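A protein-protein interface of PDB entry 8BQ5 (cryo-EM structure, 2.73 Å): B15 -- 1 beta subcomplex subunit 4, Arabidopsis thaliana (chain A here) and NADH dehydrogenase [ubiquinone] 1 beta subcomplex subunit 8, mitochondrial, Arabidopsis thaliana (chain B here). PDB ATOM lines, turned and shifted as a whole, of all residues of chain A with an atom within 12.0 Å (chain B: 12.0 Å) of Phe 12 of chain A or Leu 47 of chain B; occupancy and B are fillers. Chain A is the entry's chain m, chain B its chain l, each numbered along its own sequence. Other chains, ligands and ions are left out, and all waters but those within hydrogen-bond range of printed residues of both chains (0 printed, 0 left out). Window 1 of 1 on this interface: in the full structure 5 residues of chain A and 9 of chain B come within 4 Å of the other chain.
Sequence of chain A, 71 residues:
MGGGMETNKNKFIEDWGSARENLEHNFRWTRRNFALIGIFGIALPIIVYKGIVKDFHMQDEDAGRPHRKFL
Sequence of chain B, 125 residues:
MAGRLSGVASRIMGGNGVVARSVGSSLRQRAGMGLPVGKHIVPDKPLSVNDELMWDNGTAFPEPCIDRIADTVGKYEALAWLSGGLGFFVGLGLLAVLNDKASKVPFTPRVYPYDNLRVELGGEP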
ATOM      1  N   THR A   7      14.076   9.761  -5.487  1.00  0.00           N
ATOM      2  CA  THR A   7      14.341   8.736  -6.484  1.00  0.00           C
ATOM      3  C   THR A   7      13.046   8.086  -6.945  1.00  0.00           C
ATOM      4  O   THR A   7      12.082   7.968  -6.184  1.00  0.00           O
ATOM      5  CB  THR A   7      15.276   7.671  -5.916  1.00  0.00           C
ATOM      6  OG1 THR A   7      15.284   6.525  -6.778  1.00  0.00           O
ATOM      7  CG2 THR A   7      14.797   7.248  -4.556  1.00  0.00           C
ATOM      8  N   ASN A   8      13.024   7.673  -8.207  1.00  0.00           N
ATOM      9  CA  ASN A   8      11.920   6.883  -8.734  1.00  0.00           C
ATOM     10  C   ASN A   8      12.135   5.432  -8.325  1.00  0.00           C
ATOM     11  O   ASN A   8      12.938   4.717  -8.934  1.00  0.00           O
ATOM     12  CB  ASN A   8      11.826   7.045 -10.246  1.00  0.00           C
ATOM     13  CG  ASN A   8      11.912   8.495 -10.675  1.00  0.00           C
ATOM     14  OD1 ASN A   8      12.597   8.834 -11.639  1.00  0.00           O
ATOM     15  ND2 ASN A   8      11.217   9.365  -9.950  1.00  0.00           N
ATOM     16  N   LYS A   9      11.415   5.006  -7.289  1.00  0.00           N
ATOM     17  CA  LYS A   9      11.583   3.670  -6.737  1.00  0.00           C
ATOM     18  C   LYS A   9      11.318   2.606  -7.795  1.00  0.00           C
ATOM     19  O   LYS A   9      10.481   2.781  -8.683  1.00  0.00           O
ATOM     20  CB  LYS A   9      10.627   3.465  -5.562  1.00  0.00           C
ATOM     21  CG  LYS A   9      11.274   3.393  -4.192  1.00  0.00           C
ATOM     22  CD  LYS A   9      12.233   4.533  -3.921  1.00  0.00           C
ATOM     23  CE  LYS A   9      12.465   4.654  -2.421  1.00  0.00           C
ATOM     24  NZ  LYS A   9      13.131   5.925  -2.034  1.00  0.00           N
ATOM     25  N   ASN A  10      12.044   1.500  -7.692  1.00  0.00           N
ATOM     26  CA  ASN A  10      11.839   0.335  -8.539  1.00  0.00           C
ATOM     27  C   ASN A  10      11.357  -0.814  -7.664  1.00  0.00           C
ATOM     28  O   ASN A  10      12.002  -1.148  -6.666  1.00  0.00           O
ATOM     29  CB  ASN A  10      13.130  -0.038  -9.270  1.00  0.00           C
ATOM     30  CG  ASN A  10      12.970  -1.256 -10.147  1.00  0.00           C
ATOM     31  OD1 ASN A  10      13.341  -2.364  -9.766  1.00  0.00           O
ATOM     32  ND2 ASN A  10      12.415  -1.057 -11.335  1.00  0.00           N
ATOM     33  N   LYS A  11      10.221  -1.409  -8.037  1.00  0.00           N
ATOM     34  CA  LYS A  11       9.616  -2.445  -7.202  1.00  0.00           C
ATOM     35  C   LYS A  11      10.554  -3.633  -7.023  1.00  0.00           C
ATOM     36  O   LYS A  11      10.602  -4.238  -5.946  1.00  0.00           O
ATOM     37  CB  LYS A  11       8.284  -2.892  -7.811  1.00  0.00           C
ATOM     38  CG  LYS A  11       7.238  -3.338  -6.795  1.00  0.00           C
ATOM     39  CD  LYS A  11       6.782  -4.770  -7.039  1.00  0.00           C
ATOM     40  CE  LYS A  11       5.722  -5.199  -6.037  1.00  0.00           C
ATOM     41  NZ  LYS A  11       6.271  -5.297  -4.654  1.00  0.00           N
ATOM     42  N   PHE A  12      11.310  -3.981  -8.066  1.00  0.00           N
ATOM     43  CA  PHE A  12      12.211  -5.124  -7.964  1.00  0.00           C
ATOM     44  C   PHE A  12      13.457  -4.779  -7.160  1.00  0.00           C
ATOM     45  O   PHE A  12      13.980  -5.624  -6.423  1.00  0.00           O
ATOM     46  CB  PHE A  12      12.579  -5.622  -9.358  1.00  0.00           C
ATOM     47  CG  PHE A  12      11.396  -6.044 -10.171  1.00  0.00           C
ATOM     48  CD1 PHE A  12      10.831  -7.294  -9.999  1.00  0.00           C
ATOM     49  CD2 PHE A  12      10.840  -5.184 -11.102  1.00  0.00           C
ATOM     50  CE1 PHE A  12       9.734  -7.680 -10.742  1.00  0.00           C
ATOM     51  CE2 PHE A  12       9.744  -5.565 -11.849  1.00  0.00           C
ATOM     52  CZ  PHE A  12       9.191  -6.815 -11.668  1.00  0.00           C
ATOM     53  N   ILE A  13      13.950  -3.547  -7.286  1.00  0.00           N
ATOM     54  CA  ILE A  13      15.069  -3.115  -6.455  1.00  0.00           C
ATOM     55  C   ILE A  13      14.634  -2.997  -5.000  1.00  0.00           C
ATOM     56  O   ILE A  13      15.373  -3.375  -4.082  1.00  0.00           O
ATOM     57  CB  ILE A  13      15.660  -1.799  -6.994  1.00  0.00           C
ATOM     58  CG1 ILE A  13      16.396  -2.057  -8.310  1.00  0.00           C
ATOM     59  CG2 ILE A  13      16.608  -1.178  -5.986  1.00  0.00           C
ATOM     60  CD1 ILE A  13      16.814  -0.806  -9.037  1.00  0.00           C
ATOM     61  N   GLU A  14      13.420  -2.494  -4.765  1.00  0.00           N
ATOM     62  CA  GLU A  14      12.933  -2.362  -3.394  1.00  0.00           C
ATOM     63  C   GLU A  14      12.572  -3.711  -2.785  1.00  0.00           C
ATOM     64  O   GLU A  14      12.778  -3.927  -1.586  1.00  0.00           O
ATOM     65  CB  GLU A  14      11.743  -1.407  -3.345  1.00  0.00           C
ATOM     66  CG  GLU A  14      12.117   0.011  -3.705  1.00  0.00           C
ATOM     67  CD  GLU A  14      12.882   0.694  -2.588  1.00  0.00           C
ATOM     68  OE1 GLU A  14      12.732   0.268  -1.424  1.00  0.00           O
ATOM     69  OE2 GLU A  14      13.644   1.639  -2.873  1.00  0.00           O
ATOM     70  N   ASP A  15      12.011  -4.625  -3.580  1.00  0.00           N
ATOM     71  CA  ASP A  15      11.809  -5.986  -3.091  1.00  0.00           C
ATOM     72  C   ASP A  15      13.145  -6.655  -2.792  1.00  0.00           C
ATOM     73  O   ASP A  15      13.290  -7.349  -1.779  1.00  0.00           O
ATOM     74  CB  ASP A  15      11.011  -6.807  -4.105  1.00  0.00           C
ATOM     75  CG  ASP A  15       9.516  -6.594  -3.980  1.00  0.00           C
ATOM     76  OD1 ASP A  15       8.757  -7.558  -4.217  1.00  0.00           O
ATOM     77  OD2 ASP A  15       9.095  -5.466  -3.647  1.00  0.00           O
ATOM     78  N   TRP A  16      14.129  -6.455  -3.671  1.00  0.00           N
ATOM     79  CA  TRP A  16      15.496  -6.886  -3.393  1.00  0.00           C
ATOM     80  C   TRP A  16      15.998  -6.302  -2.081  1.00  0.00           C
ATOM     81  O   TRP A  16      16.623  -7.000  -1.273  1.00  0.00           O
ATOM     82  CB  TRP A  16      16.405  -6.462  -4.546  1.00  0.00           C
ATOM     83  CG  TRP A  16      17.781  -7.021  -4.491  1.00  0.00           C
ATOM     84  CD1 TRP A  16      18.136  -8.334  -4.475  1.00  0.00           C
ATOM     85  CD2 TRP A  16      18.998  -6.272  -4.422  1.00  0.00           C
ATOM     86  NE1 TRP A  16      19.504  -8.451  -4.416  1.00  0.00           N
ATOM     87  CE2 TRP A  16      20.055  -7.198  -4.380  1.00  0.00           C
ATOM     88  CE3 TRP A  16      19.294  -4.906  -4.395  1.00  0.00           C
ATOM     89  CZ2 TRP A  16      21.388  -6.804  -4.314  1.00  0.00           C
ATOM     90  CZ3 TRP A  16      20.616  -4.517  -4.331  1.00  0.00           C
ATOM     91  CH2 TRP A  16      21.648  -5.462  -4.292  1.00  0.00           C
ATOM     92  N   GLY A  17      15.742  -5.012  -1.857  1.00  0.00           N
ATOM     93  CA  GLY A  17      16.224  -4.369  -0.645  1.00  0.00           C
ATOM     94  C   GLY A  17      15.545  -4.887   0.607  1.00  0.00           C
ATOM     95  O   GLY A  17      16.190  -5.097   1.636  1.00  0.00           O
ATOM     96  N   SER A  18      14.228  -5.097   0.538  1.00  0.00           N
ATOM     97  CA  SER A  18      13.489  -5.537   1.716  1.00  0.00           C
ATOM     98  C   SER A  18      13.723  -7.009   2.020  1.00  0.00           C
ATOM     99  O   SER A  18      13.607  -7.427   3.177  1.00  0.00           O
ATOM    100  CB  SER A  18      11.998  -5.261   1.535  1.00  0.00           C
ATOM    101  OG  SER A  18      11.739  -3.869   1.560  1.00  0.00           O
ATOM    102  N   ALA A  19      14.045  -7.811   1.002  1.00  0.00           N
ATOM    103  CA  ALA A  19      14.382  -9.208   1.253  1.00  0.00           C
ATOM    104  C   ALA A  19      15.593  -9.316   2.166  1.00  0.00           C
ATOM    105  O   ALA A  19      15.613 -10.134   3.093  1.00  0.00           O
ATOM    106  CB  ALA A  19      14.638  -9.935  -0.067  1.00  0.00           C
ATOM    107  N   ARG A  20      16.606  -8.481   1.928  1.00  0.00           N
ATOM    108  CA  ARG A  20      17.829  -8.529   2.722  1.00  0.00           C
ATOM    109  C   ARG A  20      17.561  -8.212   4.190  1.00  0.00           C
ATOM    110  O   ARG A  20      18.134  -8.845   5.083  1.00  0.00           O
ATOM    111  CB  ARG A  20      18.859  -7.563   2.139  1.00  0.00           C
ATOM    112  CG  ARG A  20      20.170  -7.551   2.888  1.00  0.00           C
ATOM    113  CD  ARG A  20      21.030  -8.749   2.526  1.00  0.00           C
ATOM    114  NE  ARG A  20      21.053  -9.036   1.096  1.00  0.00           N
ATOM    115  CZ  ARG A  20      21.994  -8.603   0.269  1.00  0.00           C
ATOM    116  NH1 ARG A  20      22.993  -7.849   0.694  1.00  0.00           N
ATOM    117  NH2 ARG A  20      21.936  -8.943  -1.017  1.00  0.00           N
ATOM    118  N   GLU A  21      16.699  -7.230   4.461  1.00  0.00           N
ATOM    119  CA  GLU A  21      16.450  -6.795   5.831  1.00  0.00           C
ATOM    120  C   GLU A  21      15.695  -7.823   6.664  1.00  0.00           C
ATOM    121  O   GLU A  21      15.668  -7.693   7.891  1.00  0.00           O
ATOM    122  CB  GLU A  21      15.666  -5.483   5.837  1.00  0.00           C
ATOM    123  CG  GLU A  21      15.961  -4.584   4.665  1.00  0.00           C
ATOM    124  CD  GLU A  21      15.698  -3.131   4.971  1.00  0.00           C
ATOM    125  OE1 GLU A  21      14.790  -2.545   4.343  1.00  0.00           O
ATOM    126  OE2 GLU A  21      16.398  -2.571   5.839  1.00  0.00           O
ATOM    127  N   LEU A  23      16.125 -11.353   6.650  1.00  0.00           N
ATOM    128  CA  LEU A  23      16.760 -12.642   6.397  1.00  0.00           C
ATOM    129  C   LEU A  23      16.553 -13.622   7.543  1.00  0.00           C
ATOM    130  O   LEU A  23      16.539 -14.838   7.318  1.00  0.00           O
ATOM    131  CB  LEU A  23      18.252 -12.449   6.139  1.00  0.00           C
ATOM    132  CG  LEU A  23      18.833 -13.267   4.986  1.00  0.00           C
ATOM    133  CD1 LEU A  23      17.987 -13.106   3.735  1.00  0.00           C
ATOM    134  CD2 LEU A  23      20.274 -12.870   4.724  1.00  0.00           C
ATOM    135  N   LYS B  39      21.912   3.897 -22.006  1.00  0.00           N
ATOM    136  CA  LYS B  39      20.691   3.672 -21.238  1.00  0.00           C
ATOM    137  C   LYS B  39      20.960   2.553 -20.240  1.00  0.00           C
ATOM    138  O   LYS B  39      21.245   1.422 -20.645  1.00  0.00           O
ATOM    139  CB  LYS B  39      19.531   3.327 -22.165  1.00  0.00           C
ATOM    140  CG  LYS B  39      18.152   3.619 -21.599  1.00  0.00           C
ATOM    141  CD  LYS B  39      17.550   2.407 -20.924  1.00  0.00           C
ATOM    142  CE  LYS B  39      16.442   2.811 -19.964  1.00  0.00           C
ATOM    143  NZ  LYS B  39      15.592   1.652 -19.577  1.00  0.00           N
ATOM    144  N   HIS B  40      20.879   2.865 -18.949  1.00  0.00           N
ATOM    145  CA  HIS B  40      20.993   1.826 -17.935  1.00  0.00           C
ATOM    146  C   HIS B  40      19.708   1.009 -17.892  1.00  0.00           C
ATOM    147  O   HIS B  40      18.610   1.545 -18.063  1.00  0.00           O
ATOM    148  CB  HIS B  40      21.292   2.440 -16.569  1.00  0.00           C
ATOM    149  CG  HIS B  40      20.158   3.235 -16.003  1.00  0.00           C
ATOM    150  ND1 HIS B  40      19.348   2.761 -14.995  1.00  0.00           N
ATOM    151  CD2 HIS B  40      19.692   4.467 -16.313  1.00  0.00           C
ATOM    152  CE1 HIS B  40      18.435   3.670 -14.702  1.00  0.00           C
ATOM    153  NE2 HIS B  40      18.623   4.716 -15.488  1.00  0.00           N
ATOM    154  N   ILE B  41      19.848  -0.296 -17.662  1.00  0.00           N
ATOM    155  CA  ILE B  41      18.717  -1.203 -17.808  1.00  0.00           C
ATOM    156  C   ILE B  41      17.978  -1.314 -16.482  1.00  0.00           C
ATOM    157  O   ILE B  41      18.523  -1.799 -15.481  1.00  0.00           O
ATOM    158  CB  ILE B  41      19.173  -2.584 -18.312  1.00  0.00           C
ATOM    159  CG1 ILE B  41      20.061  -2.488 -19.565  1.00  0.00           C
ATOM    160  CG2 ILE B  41      17.967  -3.457 -18.623  1.00  0.00           C
ATOM    161  CD1 ILE B  41      21.519  -2.082 -19.346  1.00  0.00           C
ATOM    162  N   VAL B  42      16.731  -0.856 -16.468  1.00  0.00           N
ATOM    163  CA  VAL B  42      15.879  -0.928 -15.286  1.00  0.00           C
ATOM    164  C   VAL B  42      15.441  -2.380 -15.114  1.00  0.00           C
ATOM    165  O   VAL B  42      14.998  -2.999 -16.094  1.00  0.00           O
ATOM    166  CB  VAL B  42      14.669   0.004 -15.414  1.00  0.00           C
ATOM    167  CG1 VAL B  42      13.665  -0.257 -14.307  1.00  0.00           C
ATOM    168  CG2 VAL B  42      15.126   1.453 -15.384  1.00  0.00           C
ATOM    169  N   PRO B  43      15.571  -2.963 -13.923  1.00  0.00           N
ATOM    170  CA  PRO B  43      15.180  -4.366 -13.747  1.00  0.00           C
ATOM    171  C   PRO B  43      13.696  -4.579 -14.006  1.00  0.00           C
ATOM    172  O   PRO B  43      12.845  -3.815 -13.548  1.00  0.00           O
ATOM    173  CB  PRO B  43      15.545  -4.656 -12.287  1.00  0.00           C
ATOM    174  CG  PRO B  43      16.577  -3.640 -11.944  1.00  0.00           C
ATOM    175  CD  PRO B  43      16.190  -2.409 -12.708  1.00  0.00           C
ATOM    176  N   ASP B  44      13.399  -5.641 -14.754  1.00  0.00           N
ATOM    177  CA  ASP B  44      12.036  -6.084 -15.000  1.00  0.00           C
ATOM    178  C   ASP B  44      11.759  -7.455 -14.402  1.00  0.00           C
ATOM    179  O   ASP B  44      10.625  -7.940 -14.491  1.00  0.00           O
ATOM    180  CB  ASP B  44      11.747  -6.105 -16.508  1.00  0.00           C
ATOM    181  CG  ASP B  44      12.842  -6.797 -17.305  1.00  0.00           C
ATOM    182  OD1 ASP B  44      12.906  -6.592 -18.535  1.00  0.00           O
ATOM    183  OD2 ASP B  44      13.640  -7.546 -16.702  1.00  0.00           O
ATOM    184  N   LYS B  45      12.759  -8.087 -13.805  1.00  0.00           N
ATOM    185  CA  LYS B  45      12.670  -9.395 -13.177  1.00  0.00           C
ATOM    186  C   LYS B  45      13.217  -9.284 -11.765  1.00  0.00           C
ATOM    187  O   LYS B  45      14.007  -8.381 -11.469  1.00  0.00           O
ATOM    188  CB  LYS B  45      13.464 -10.443 -13.974  1.00  0.00           C
ATOM    189  CG  LYS B  45      12.794 -11.806 -14.086  1.00  0.00           C
ATOM    190  CD  LYS B  45      13.819 -12.926 -14.202  1.00  0.00           C
ATOM    191  CE  LYS B  45      14.767 -12.941 -13.012  1.00  0.00           C
ATOM    192  NZ  LYS B  45      15.434 -14.261 -12.843  1.00  0.00           N
ATOM    193  N   PRO B  46      12.793 -10.164 -10.859  1.00  0.00           N
ATOM    194  CA  PRO B  46      13.347 -10.137  -9.500  1.00  0.00           C
ATOM    195  C   PRO B  46      14.862 -10.292  -9.505  1.00  0.00           C
ATOM    196  O   PRO B  46      15.422 -11.094 -10.255  1.00  0.00           O
ATOM    197  CB  PRO B  46      12.655 -11.318  -8.817  1.00  0.00           C
ATOM    198  CG  PRO B  46      11.346 -11.422  -9.523  1.00  0.00           C
ATOM    199  CD  PRO B  46      11.616 -11.045 -10.953  1.00  0.00           C
ATOM    200  N   LEU B  47      15.518  -9.506  -8.659  1.00  0.00           N
ATOM    201  CA  LEU B  47      16.968  -9.537  -8.564  1.00  0.00           C
ATOM    202  C   LEU B  47      17.416 -10.705  -7.696  1.00  0.00           C
ATOM    203  O   LEU B  47      16.750 -11.084  -6.727  1.00  0.00           O
ATOM    204  CB  LEU B  47      17.501  -8.222  -7.987  1.00  0.00           C
ATOM    205  CG  LEU B  47      17.453  -6.924  -8.806  1.00  0.00           C
ATOM    206  CD1 LEU B  47      16.035  -6.443  -9.041  1.00  0.00           C
ATOM    207  CD2 LEU B  47      18.256  -5.831  -8.116  1.00  0.00           C
ATOM    208  N   SER B  48      18.555 -11.287  -8.058  1.00  0.00           N
ATOM    209  CA  SER B  48      19.117 -12.376  -7.281  1.00  0.00           C
ATOM    210  C   SER B  48      19.811 -11.833  -6.035  1.00  0.00           C
ATOM    211  O   SER B  48      20.063 -10.633  -5.899  1.00  0.00           O
ATOM    212  CB  SER B  48      20.096 -13.190  -8.124  1.00  0.00           C
ATOM    213  OG  SER B  48      21.016 -13.881  -7.299  1.00  0.00           O
ATOM    214  N   VAL B  49      20.110 -12.739  -5.105  1.00  0.00           N
ATOM    215  CA  VAL B  49      20.740 -12.323  -3.856  1.00  0.00           C
ATOM    216  C   VAL B  49      22.191 -11.907  -4.088  1.00  0.00           C
ATOM    217  O   VAL B  49      22.668 -10.930  -3.498  1.00  0.00           O
ATOM    218  CB  VAL B  49      20.593 -13.428  -2.793  1.00  0.00           C
ATOM    219  CG1 VAL B  49      19.133 -13.830  -2.679  1.00  0.00           C
ATOM    220  CG2 VAL B  49      21.424 -14.644  -3.145  1.00  0.00           C
ATOM    221  N   ASN B  50      22.913 -12.622  -4.951  1.00  0.00           N
ATOM    222  CA  ASN B  50      24.283 -12.248  -5.309  1.00  0.00           C
ATOM    223  C   ASN B  50      24.277 -11.428  -6.599  1.00  0.00           C
ATOM    224  O   ASN B  50      24.919 -11.762  -7.594  1.00  0.00           O
ATOM    225  CB  ASN B  50      25.164 -13.489  -5.444  1.00  0.00           C
ATOM    226  CG  ASN B  50      25.377 -14.208  -4.126  1.00  0.00           C
ATOM    227  OD1 ASN B  50      24.486 -14.262  -3.284  1.00  0.00           O
ATOM    228  ND2 ASN B  50      26.569 -14.766  -3.944  1.00  0.00           N
ATOM    229  N   ASP B  51      23.529 -10.327  -6.560  1.00  0.00           N
ATOM    230  CA  ASP B  51      23.426  -9.425  -7.696  1.00  0.00           C
ATOM    231  C   ASP B  51      24.369  -8.233  -7.560  1.00  0.00           C
ATOM    232  O   ASP B  51      24.752  -7.637  -8.572  1.00  0.00           O
ATOM    233  CB  ASP B  51      21.963  -8.959  -7.838  1.00  0.00           C
ATOM    234  CG  ASP B  51      21.730  -7.977  -8.987  1.00  0.00           C
ATOM    235  OD1 ASP B  51      22.645  -7.634  -9.752  1.00  0.00           O
ATOM    236  OD2 ASP B  51      20.575  -7.548  -9.144  1.00  0.00           O
ATOM    237  N   GLU B  52      24.808  -7.909  -6.343  1.00  0.00           N
ATOM    238  CA  GLU B  52      25.682  -6.759  -6.153  1.00  0.00           C
ATOM    239  C   GLU B  52      27.090  -6.996  -6.686  1.00  0.00           C
ATOM    240  O   GLU B  52      27.854  -6.035  -6.823  1.00  0.00           O
ATOM    241  CB  GLU B  52      25.744  -6.397  -4.669  1.00  0.00           C
ATOM    242  CG  GLU B  52      26.563  -7.367  -3.832  1.00  0.00           C
ATOM    243  CD  GLU B  52      25.708  -8.212  -2.911  1.00  0.00           C
ATOM    244  OE1 GLU B  52      25.716  -7.961  -1.688  1.00  0.00           O
ATOM    245  OE2 GLU B  52      25.029  -9.131  -3.412  1.00  0.00           O
ATOM    246  N   LEU B  53      27.450  -8.244  -6.990  1.00  0.00           N
ATOM    247  CA  LEU B  53      28.803  -8.577  -7.415  1.00  0.00           C
ATOM    248  C   LEU B  53      28.912  -8.987  -8.878  1.00  0.00           C
ATOM    249  O   LEU B  53      29.996  -8.850  -9.459  1.00  0.00           O
ATOM    250  CB  LEU B  53      29.386  -9.681  -6.516  1.00  0.00           C
ATOM    251  CG  LEU B  53      28.613 -10.958  -6.151  1.00  0.00           C
ATOM    252  CD1 LEU B  53      28.348 -11.869  -7.338  1.00  0.00           C
ATOM    253  CD2 LEU B  53      29.363 -11.718  -5.071  1.00  0.00           C
ATOM    254  N   MET B  54      27.839  -9.476  -9.491  1.00  0.00           N
ATOM    255  CA  MET B  54      27.899  -9.925 -10.881  1.00  0.00           C
ATOM    256  C   MET B  54      27.855  -8.754 -11.857  1.00  0.00           C
ATOM    257  O   MET B  54      28.179  -8.909 -13.037  1.00  0.00           O
ATOM    258  CB  MET B  54      26.756 -10.898 -11.182  1.00  0.00           C
ATOM    259  CG  MET B  54      26.991 -12.315 -10.682  1.00  0.00           C
ATOM    260  SD  MET B  54      27.822 -13.371 -11.888  1.00  0.00           S
ATOM    261  CE  MET B  54      27.314 -12.606 -13.425  1.00  0.00           C
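Among the printed residues, pairs that only touch across the chains: Asn 10 of chain A with Val 42 of chain B (3.3 Å), Asn 10 of chain A with Pro 43 of chain B (3.6 Å), Phe 12 of chain A with Pro 43 of chain B (3.4 Å), Phe 12 of chain A with Asp 44 of chain B (3.4 Å), Phe 12 of chain A with Lys 45 of chain B (3.6 Å), Phe 12 of chain A with Pro 46 of chain B (3.6 Å), Phe 12 of chain A with Leu 47 of chain B (3.4 Å), Ile 13 of chain A with Pro 43 of chain B (3.97 Å), Ile 13 of chain A with Leu 47 of chain B (3.98 Å) and Trp 16 of chain A with Leu 47 of chain B (3.6 Å).
Lys 9 of chain A touches none of the printed residues of chain B. No residue of chain B comes within 4 Å of Lys 11 of chain A. Of the printed residues of chain B, Phe 12 of chain A touches Pro 43, Asp 44, Lys 45, Pro 46 and Leu 47. Of chain B, only Pro 43 and Leu 47 come within 4 Å of Ile 13 of chain A. No residue of chain B comes within 4 Å of Glu 14 of chain A. No residue of chain B comes within 4 Å of Asp 15 of chain A. Of the printed residues of chain B, Arg 20 of chain A touches Val 49 (3.3 Å) and Glu 52 (3.6 Å). Of the printed residues of chain A, Val 42 of chain B touches Asn 10. Asp 44 of chain B touches one residue of chain A. Lys 45 of chain B touches one residue of chain A. Of chain A, only Phe 12 (3.4 Å), Ile 13 (3.98 Å) and Trp 16 (3.6 Å) come within 4 Å of Leu 47 of chain B. Ser 48 of chain B touches one residue of chain A. Val 49 of chain B touches one residue of chain A. No residue of chain A comes within 4 Å of Asp 51 of chain B. Of the printed residues of chain A, Glu 52 of chain B touches Arg 20. The nearest residue of chain A that does not touch Leu 47 of chain B is Asn 10 of chain A (4.9 Å). The nearest printed residue of chain A that does not touch Glu 52 of chain B is Trp 16 of chain A (4.1 Å).
Of the 16 printed residues of chain B, 9 touch a printed residue of chain A. Hydrophobic or aromatic side chains of chain A that line the printed part of chain B: Phe 12, Ile 13 and Trp 16.
OG of Ser 48 of chain B lies within hydrogen-bond range of N of Asn 50 of chain B, 3.3 Å away. N of Phe 12 of chain A sits at hydrogen-bond distance from OD1 of Asn 10 of chain A, 3.1 Å away. The side-chain amide oxygen (OD1) of Asn 10 of chain A sits at hydrogen-bond distance from the backbone NH (N) of Ile 13 of chain A (2.8 Å).
O of Val 49 of chain B sits at hydrogen-bond distance from NH2 of Arg 20 of chain A, 3.3 Å away. The side-chain carboxylate (OE1) of Glu 52 of chain B is in salt-bridge range of the guanidinium group (NH1) of Arg 20 of chain A (3.6 Å). O of Ser 48 of chain B lies within hydrogen-bond range of NE1 of Trp 16 of chain A, 2.7 Å away.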
